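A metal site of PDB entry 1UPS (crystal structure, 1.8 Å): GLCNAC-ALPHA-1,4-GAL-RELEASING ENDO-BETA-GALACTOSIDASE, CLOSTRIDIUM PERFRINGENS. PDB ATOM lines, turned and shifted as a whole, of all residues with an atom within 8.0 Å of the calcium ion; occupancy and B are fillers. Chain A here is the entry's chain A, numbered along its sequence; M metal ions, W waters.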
ATOM      1  N   ALA A  22      -3.261 -15.785 -11.956  1.00  0.00           N
ATOM      2  CA  ALA A  22      -4.237 -15.063 -12.761  1.00  0.00           C
ATOM      3  C   ALA A  22      -4.239 -15.554 -14.223  1.00  0.00           C
ATOM      4  O   ALA A  22      -3.154 -15.787 -14.822  1.00  0.00           O
ATOM      5  CB  ALA A  22      -3.951 -13.570 -12.690  1.00  0.00           C
ATOM      6  N   ASP A  36     -12.996  -5.305 -14.994  1.00  0.00           N
ATOM      7  CA  ASP A  36     -12.535  -4.411 -13.967  1.00  0.00           C
ATOM      8  C   ASP A  36     -11.385  -5.116 -13.262  1.00  0.00           C
ATOM      9  O   ASP A  36     -11.575  -6.185 -12.665  1.00  0.00           O
ATOM     10  CB  ASP A  36     -13.654  -4.053 -12.987  1.00  0.00           C
ATOM     11  CG  ASP A  36     -13.327  -2.833 -12.172  1.00  0.00           C
ATOM     12  OD1 ASP A  36     -14.239  -2.080 -11.770  1.00  0.00           O
ATOM     13  OD2 ASP A  36     -12.137  -2.546 -11.915  1.00  0.00           O
ATOM     14  N   GLU A  37     -10.193  -4.524 -13.363  1.00  0.00           N
ATOM     15  CA  GLU A  37      -9.000  -5.085 -12.720  1.00  0.00           C
ATOM     16  C   GLU A  37      -8.862  -4.630 -11.258  1.00  0.00           C
ATOM     17  O   GLU A  37      -7.924  -5.029 -10.555  1.00  0.00           O
ATOM     18  CB  GLU A  37      -7.744  -4.739 -13.548  1.00  0.00           C
ATOM     19  CG  GLU A  37      -7.837  -5.229 -15.008  1.00  0.00           C
ATOM     20  CD  GLU A  37      -7.867  -6.749 -15.129  1.00  0.00           C
ATOM     21  OE1 GLU A  37      -8.642  -7.247 -15.980  1.00  0.00           O
ATOM     22  OE2 GLU A  37      -7.146  -7.440 -14.373  1.00  0.00           O
ATOM     23  N   PHE A  38      -9.836  -3.834 -10.786  1.00  0.00           N
ATOM     24  CA  PHE A  38      -9.968  -3.475  -9.366  1.00  0.00           C
ATOM     25  C   PHE A  38      -8.666  -2.991  -8.719  1.00  0.00           C
ATOM     26  O   PHE A  38      -8.347  -3.375  -7.606  1.00  0.00           O
ATOM     27  CB  PHE A  38     -10.554  -4.627  -8.546  1.00  0.00           C
ATOM     28  CG  PHE A  38     -12.013  -4.940  -8.853  1.00  0.00           C
ATOM     29  CD1 PHE A  38     -12.418  -6.258  -9.095  1.00  0.00           C
ATOM     30  CD2 PHE A  38     -12.983  -3.929  -8.852  1.00  0.00           C
ATOM     31  CE1 PHE A  38     -13.765  -6.568  -9.367  1.00  0.00           C
ATOM     32  CE2 PHE A  38     -14.350  -4.222  -9.099  1.00  0.00           C
ATOM     33  CZ  PHE A  38     -14.745  -5.528  -9.364  1.00  0.00           C
ATOM     34  N   ASN A  39      -7.907  -2.159  -9.400  1.00  0.00           N
ATOM     35  CA  ASN A  39      -6.647  -1.714  -8.783  1.00  0.00           C
ATOM     36  C   ASN A  39      -6.811  -0.535  -7.819  1.00  0.00           C
ATOM     37  O   ASN A  39      -5.935  -0.297  -6.942  1.00  0.00           O
ATOM     38  CB  ASN A  39      -5.562  -1.533  -9.840  1.00  0.00           C
ATOM     39  CG  ASN A  39      -5.284  -2.823 -10.629  1.00  0.00           C
ATOM     40  OD1 ASN A  39      -5.263  -3.939 -10.080  1.00  0.00           O
ATOM     41  ND2 ASN A  39      -5.087  -2.673 -11.942  1.00  0.00           N
ATOM     42  N   GLY A  40      -7.940   0.167  -7.926  1.00  0.00           N
ATOM     43  CA  GLY A  40      -8.229   1.301  -7.058  1.00  0.00           C
ATOM     44  C   GLY A  40      -7.364   2.497  -7.379  1.00  0.00           C
ATOM     45  O   GLY A  40      -6.648   2.464  -8.378  1.00  0.00           O
ATOM     46  N   PHE A  69      -9.426  -0.635  -1.554  1.00  0.00           N
ATOM     47  CA  PHE A  69      -8.642  -1.389  -2.518  1.00  0.00           C
ATOM     48  C   PHE A  69      -7.314  -1.693  -1.864  1.00  0.00           C
ATOM     49  O   PHE A  69      -6.704  -0.795  -1.272  1.00  0.00           O
ATOM     50  CB  PHE A  69      -8.458  -0.575  -3.802  1.00  0.00           C
ATOM     51  CG  PHE A  69      -9.750  -0.395  -4.562  1.00  0.00           C
ATOM     52  CD1 PHE A  69     -10.109  -1.294  -5.571  1.00  0.00           C
ATOM     53  CD2 PHE A  69     -10.608   0.663  -4.238  1.00  0.00           C
ATOM     54  CE1 PHE A  69     -11.335  -1.149  -6.250  1.00  0.00           C
ATOM     55  CE2 PHE A  69     -11.821   0.816  -4.917  1.00  0.00           C
ATOM     56  CZ  PHE A  69     -12.172  -0.084  -5.931  1.00  0.00           C
ATOM     57  N   GLU A  70      -6.881  -2.958  -1.921  1.00  0.00           N
ATOM     58  CA  GLU A  70      -5.657  -3.394  -1.235  1.00  0.00           C
ATOM     59  C   GLU A  70      -4.954  -4.437  -2.109  1.00  0.00           C
ATOM     60  O   GLU A  70      -5.575  -5.430  -2.506  1.00  0.00           O
ATOM     61  CB  GLU A  70      -5.977  -3.931   0.186  1.00  0.00           C
ATOM     62  CG  GLU A  70      -4.780  -4.470   0.978  1.00  0.00           C
ATOM     63  CD  GLU A  70      -5.118  -4.839   2.433  1.00  0.00           C
ATOM     64  OE1 GLU A  70      -4.267  -5.494   3.130  1.00  0.00           O
ATOM     65  OE2 GLU A  70      -6.213  -4.453   2.917  1.00  0.00           O
ATOM     66  N   ASN A  71      -3.686  -4.181  -2.429  1.00  0.00           N
ATOM     67  CA  ASN A  71      -2.860  -5.166  -3.149  1.00  0.00           C
ATOM     68  C   ASN A  71      -3.502  -5.613  -4.469  1.00  0.00           C
ATOM     69  O   ASN A  71      -3.563  -6.811  -4.785  1.00  0.00           O
ATOM     70  CB  ASN A  71      -2.592  -6.357  -2.210  1.00  0.00           C
ATOM     71  CG  ASN A  71      -1.469  -7.268  -2.689  1.00  0.00           C
ATOM     72  OD1 ASN A  71      -0.378  -6.817  -3.060  1.00  0.00           O
ATOM     73  ND2 ASN A  71      -1.748  -8.567  -2.685  1.00  0.00           N
ATOM     74  N   GLY A  72      -3.990  -4.647  -5.246  1.00  0.00           N
ATOM     75  CA  GLY A  72      -4.631  -4.904  -6.520  1.00  0.00           C
ATOM     76  C   GLY A  72      -6.029  -5.531  -6.480  1.00  0.00           C
ATOM     77  O   GLY A  72      -6.508  -5.985  -7.524  1.00  0.00           O
ATOM     78  N   SER A  73      -6.680  -5.524  -5.319  1.00  0.00           N
ATOM     79  CA  SER A  73      -8.011  -6.148  -5.178  1.00  0.00           C
ATOM     80  C   SER A  73      -9.029  -5.186  -4.616  1.00  0.00           C
ATOM     81  O   SER A  73      -8.688  -4.295  -3.824  1.00  0.00           O
ATOM     82  CB  SER A  73      -7.937  -7.359  -4.234  1.00  0.00           C
ATOM     83  OG  SER A  73      -7.217  -8.425  -4.846  1.00  0.00           O
ATOM     84  N   LEU A  74     -10.282  -5.353  -5.021  1.00  0.00           N
ATOM     85  CA  LEU A  74     -11.380  -4.747  -4.257  1.00  0.00           C
ATOM     86  C   LEU A  74     -11.585  -5.567  -2.969  1.00  0.00           C
ATOM     87  O   LEU A  74     -11.765  -6.795  -3.020  1.00  0.00           O
ATOM     88  CB  LEU A  74     -12.678  -4.760  -5.091  1.00  0.00           C
ATOM     89  CG  LEU A  74     -13.980  -4.405  -4.358  1.00  0.00           C
ATOM     90  CD1 LEU A  74     -13.990  -2.920  -4.016  1.00  0.00           C
ATOM     91  CD2 LEU A  74     -15.173  -4.787  -5.254  1.00  0.00           C
ATOM     92  N   ARG A 134     -11.344 -13.627  -9.955  1.00  0.00           N
ATOM     93  CA  ARG A 134     -10.281 -14.255  -9.209  1.00  0.00           C
ATOM     94  C   ARG A 134     -10.400 -13.650  -7.813  1.00  0.00           C
ATOM     95  O   ARG A 134     -10.414 -12.435  -7.677  1.00  0.00           O
ATOM     96  CB  ARG A 134      -8.918 -13.953  -9.840  1.00  0.00           C
ATOM     97  CG  ARG A 134      -7.737 -14.532  -9.091  1.00  0.00           C
ATOM     98  CD  ARG A 134      -6.446 -14.508  -9.946  1.00  0.00           C
ATOM     99  NE  ARG A 134      -5.295 -15.111  -9.292  1.00  0.00           N
ATOM    100  CZ  ARG A 134      -4.409 -14.445  -8.546  1.00  0.00           C
ATOM    101  NH1 ARG A 134      -4.559 -13.144  -8.334  1.00  0.00           N
ATOM    102  NH2 ARG A 134      -3.351 -15.075  -8.017  1.00  0.00           N
ATOM    103  N   TYR A 214      -5.937 -16.930  -3.478  1.00  0.00           N
ATOM    104  CA  TYR A 214      -6.745 -16.535  -4.627  1.00  0.00           C
ATOM    105  C   TYR A 214      -7.023 -17.766  -5.477  1.00  0.00           C
ATOM    106  O   TYR A 214      -6.086 -18.558  -5.767  1.00  0.00           O
ATOM    107  CB  TYR A 214      -6.026 -15.508  -5.484  1.00  0.00           C
ATOM    108  CG  TYR A 214      -6.091 -14.131  -4.879  1.00  0.00           C
ATOM    109  CD1 TYR A 214      -7.196 -13.292  -5.103  1.00  0.00           C
ATOM    110  CD2 TYR A 214      -5.054 -13.672  -4.067  1.00  0.00           C
ATOM    111  CE1 TYR A 214      -7.239 -11.992  -4.552  1.00  0.00           C
ATOM    112  CE2 TYR A 214      -5.093 -12.393  -3.508  1.00  0.00           C
ATOM    113  CZ  TYR A 214      -6.193 -11.562  -3.741  1.00  0.00           C
ATOM    114  OH  TYR A 214      -6.213 -10.302  -3.167  1.00  0.00           O
ATOM    115  N   ILE A 271     -11.353  -9.289  -4.185  1.00  0.00           N
ATOM    116  CA  ILE A 271     -11.559  -9.660  -5.593  1.00  0.00           C
ATOM    117  C   ILE A 271     -10.491  -8.991  -6.463  1.00  0.00           C
ATOM    118  O   ILE A 271     -10.454  -7.772  -6.566  1.00  0.00           O
ATOM    119  CB  ILE A 271     -12.969  -9.260  -6.073  1.00  0.00           C
ATOM    120  CG1 ILE A 271     -14.045  -9.813  -5.106  1.00  0.00           C
ATOM    121  CG2 ILE A 271     -13.235  -9.781  -7.491  1.00  0.00           C
ATOM    122  CD1 ILE A 271     -15.146  -8.824  -4.843  1.00  0.00           C
ATOM    123  N   ASP A 272      -9.665  -9.813  -7.118  1.00  0.00           N
ATOM    124  CA  ASP A 272      -8.555  -9.315  -7.935  1.00  0.00           C
ATOM    125  C   ASP A 272      -9.045  -8.695  -9.237  1.00  0.00           C
ATOM    126  O   ASP A 272      -8.554  -7.623  -9.662  1.00  0.00           O
ATOM    127  CB  ASP A 272      -7.564 -10.466  -8.194  1.00  0.00           C
ATOM    128  CG  ASP A 272      -6.376 -10.058  -9.047  1.00  0.00           C
ATOM    129  OD1 ASP A 272      -5.791 -10.962  -9.673  1.00  0.00           O
ATOM    130  OD2 ASP A 272      -5.970  -8.867  -9.143  1.00  0.00           O
ATOM    131  N   TYR A 273     -10.004  -9.343  -9.888  1.00  0.00           N
ATOM    132  CA  TYR A 273     -10.564  -8.844 -11.138  1.00  0.00           C
ATOM    133  C   TYR A 273     -11.889  -9.527 -11.434  1.00  0.00           C
ATOM    134  O   TYR A 273     -12.190 -10.585 -10.873  1.00  0.00           O
ATOM    135  CB  TYR A 273      -9.607  -9.076 -12.341  1.00  0.00           C
ATOM    136  CG  TYR A 273      -9.296 -10.528 -12.701  1.00  0.00           C
ATOM    137  CD1 TYR A 273     -10.228 -11.329 -13.392  1.00  0.00           C
ATOM    138  CD2 TYR A 273      -8.033 -11.080 -12.449  1.00  0.00           C
ATOM    139  CE1 TYR A 273      -9.945 -12.651 -13.733  1.00  0.00           C
ATOM    140  CE2 TYR A 273      -7.726 -12.397 -12.812  1.00  0.00           C
ATOM    141  CZ  TYR A 273      -8.677 -13.158 -13.456  1.00  0.00           C
ATOM    142  OH  TYR A 273      -8.360 -14.452 -13.802  1.00  0.00           O
ATOM    143  N   MET A 274     -12.667  -8.883 -12.308  1.00  0.00           N
ATOM    144  CA  MET A 274     -13.819  -9.495 -12.960  1.00  0.00           C
ATOM    145  C   MET A 274     -13.676  -9.266 -14.462  1.00  0.00           C
ATOM    146  O   MET A 274     -13.394  -8.145 -14.897  1.00  0.00           O
ATOM    147  CB  MET A 274     -15.138  -8.867 -12.473  1.00  0.00           C
ATOM    148  CG  MET A 274     -16.371  -9.404 -13.217  1.00  0.00           C
ATOM    149  SD  MET A 274     -17.882  -8.565 -12.685  1.00  0.00           S
ATOM    150  CE  MET A 274     -18.960  -8.891 -14.082  1.00  0.00           C
ATOM    151  N   ARG A 275     -13.856 -10.320 -15.255  1.00  0.00           N
ATOM    152  CA  ARG A 275     -13.759 -10.227 -16.702  1.00  0.00           C
ATOM    153  C   ARG A 275     -14.916 -10.986 -17.327  1.00  0.00           C
ATOM    154  O   ARG A 275     -15.340 -12.027 -16.805  1.00  0.00           O
ATOM    155  CB  ARG A 275     -12.416 -10.827 -17.189  1.00  0.00           C
ATOM    156  CG  ARG A 275     -11.188 -10.038 -16.687  1.00  0.00           C
ATOM    157  CD  ARG A 275      -9.841 -10.632 -17.128  1.00  0.00           C
ATOM    158  NE  ARG A 275      -8.732 -10.039 -16.386  1.00  0.00           N
ATOM    159  CZ  ARG A 275      -7.582 -10.649 -16.146  1.00  0.00           C
ATOM    160  NH1 ARG A 275      -7.351 -11.884 -16.613  1.00  0.00           N
ATOM    161  NH2 ARG A 275      -6.632 -10.031 -15.446  1.00  0.00           N
HETATM  162 CA    CA M   1      -6.409  -6.624  -9.800  1.00  0.00          CA
HETATM  163  O   HOH W   1      -5.970  -7.501 -11.974  1.00  0.00           O
HETATM  164  O   HOH W   2      -3.960  -7.012  -9.594  1.00  0.00           O
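Four residues have an atom within 4 Å of the calcium ion: Glu 37, Asn 39, Gly 72 and Asp 272.
The nearest printed residue that does not touch the calcium ion is Phe 38 (4.4 Å).
The side-chain amide oxygen (OD1) of Asn 39 sits close to the backbone carbonyl oxygen (O) of Glu 37, at 2.9 Å.
The side-chain carboxylate (OE1) of Glu 37 lies within salt-bridge range of the guanidinium group (NE) of Arg 275 (2.8 Å).
The side-chain carboxylate of Asp 272 lies within salt-bridge range of the guanidinium group of Arg 134, 2.8 Å away.
The calcium ion is bound by the backbone carbonyl oxygen (O) of Glu 37, 2.3 Å away.
The calcium ion is bound by O of Gly 72 (2.4 Å).
The calcium ion is bound by O of Asp 272.
The calcium ion is bound by OD2 of Asp 272, 2.4 Å away.
The calcium ion is bound by water W1 (2.4 Å).
Water W2 is bound to the calcium ion.
The calcium ion has six donor atoms within binding distance.
Slightly farther from the calcium ion lies OD1 of Asn 39 (2.9 Å).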
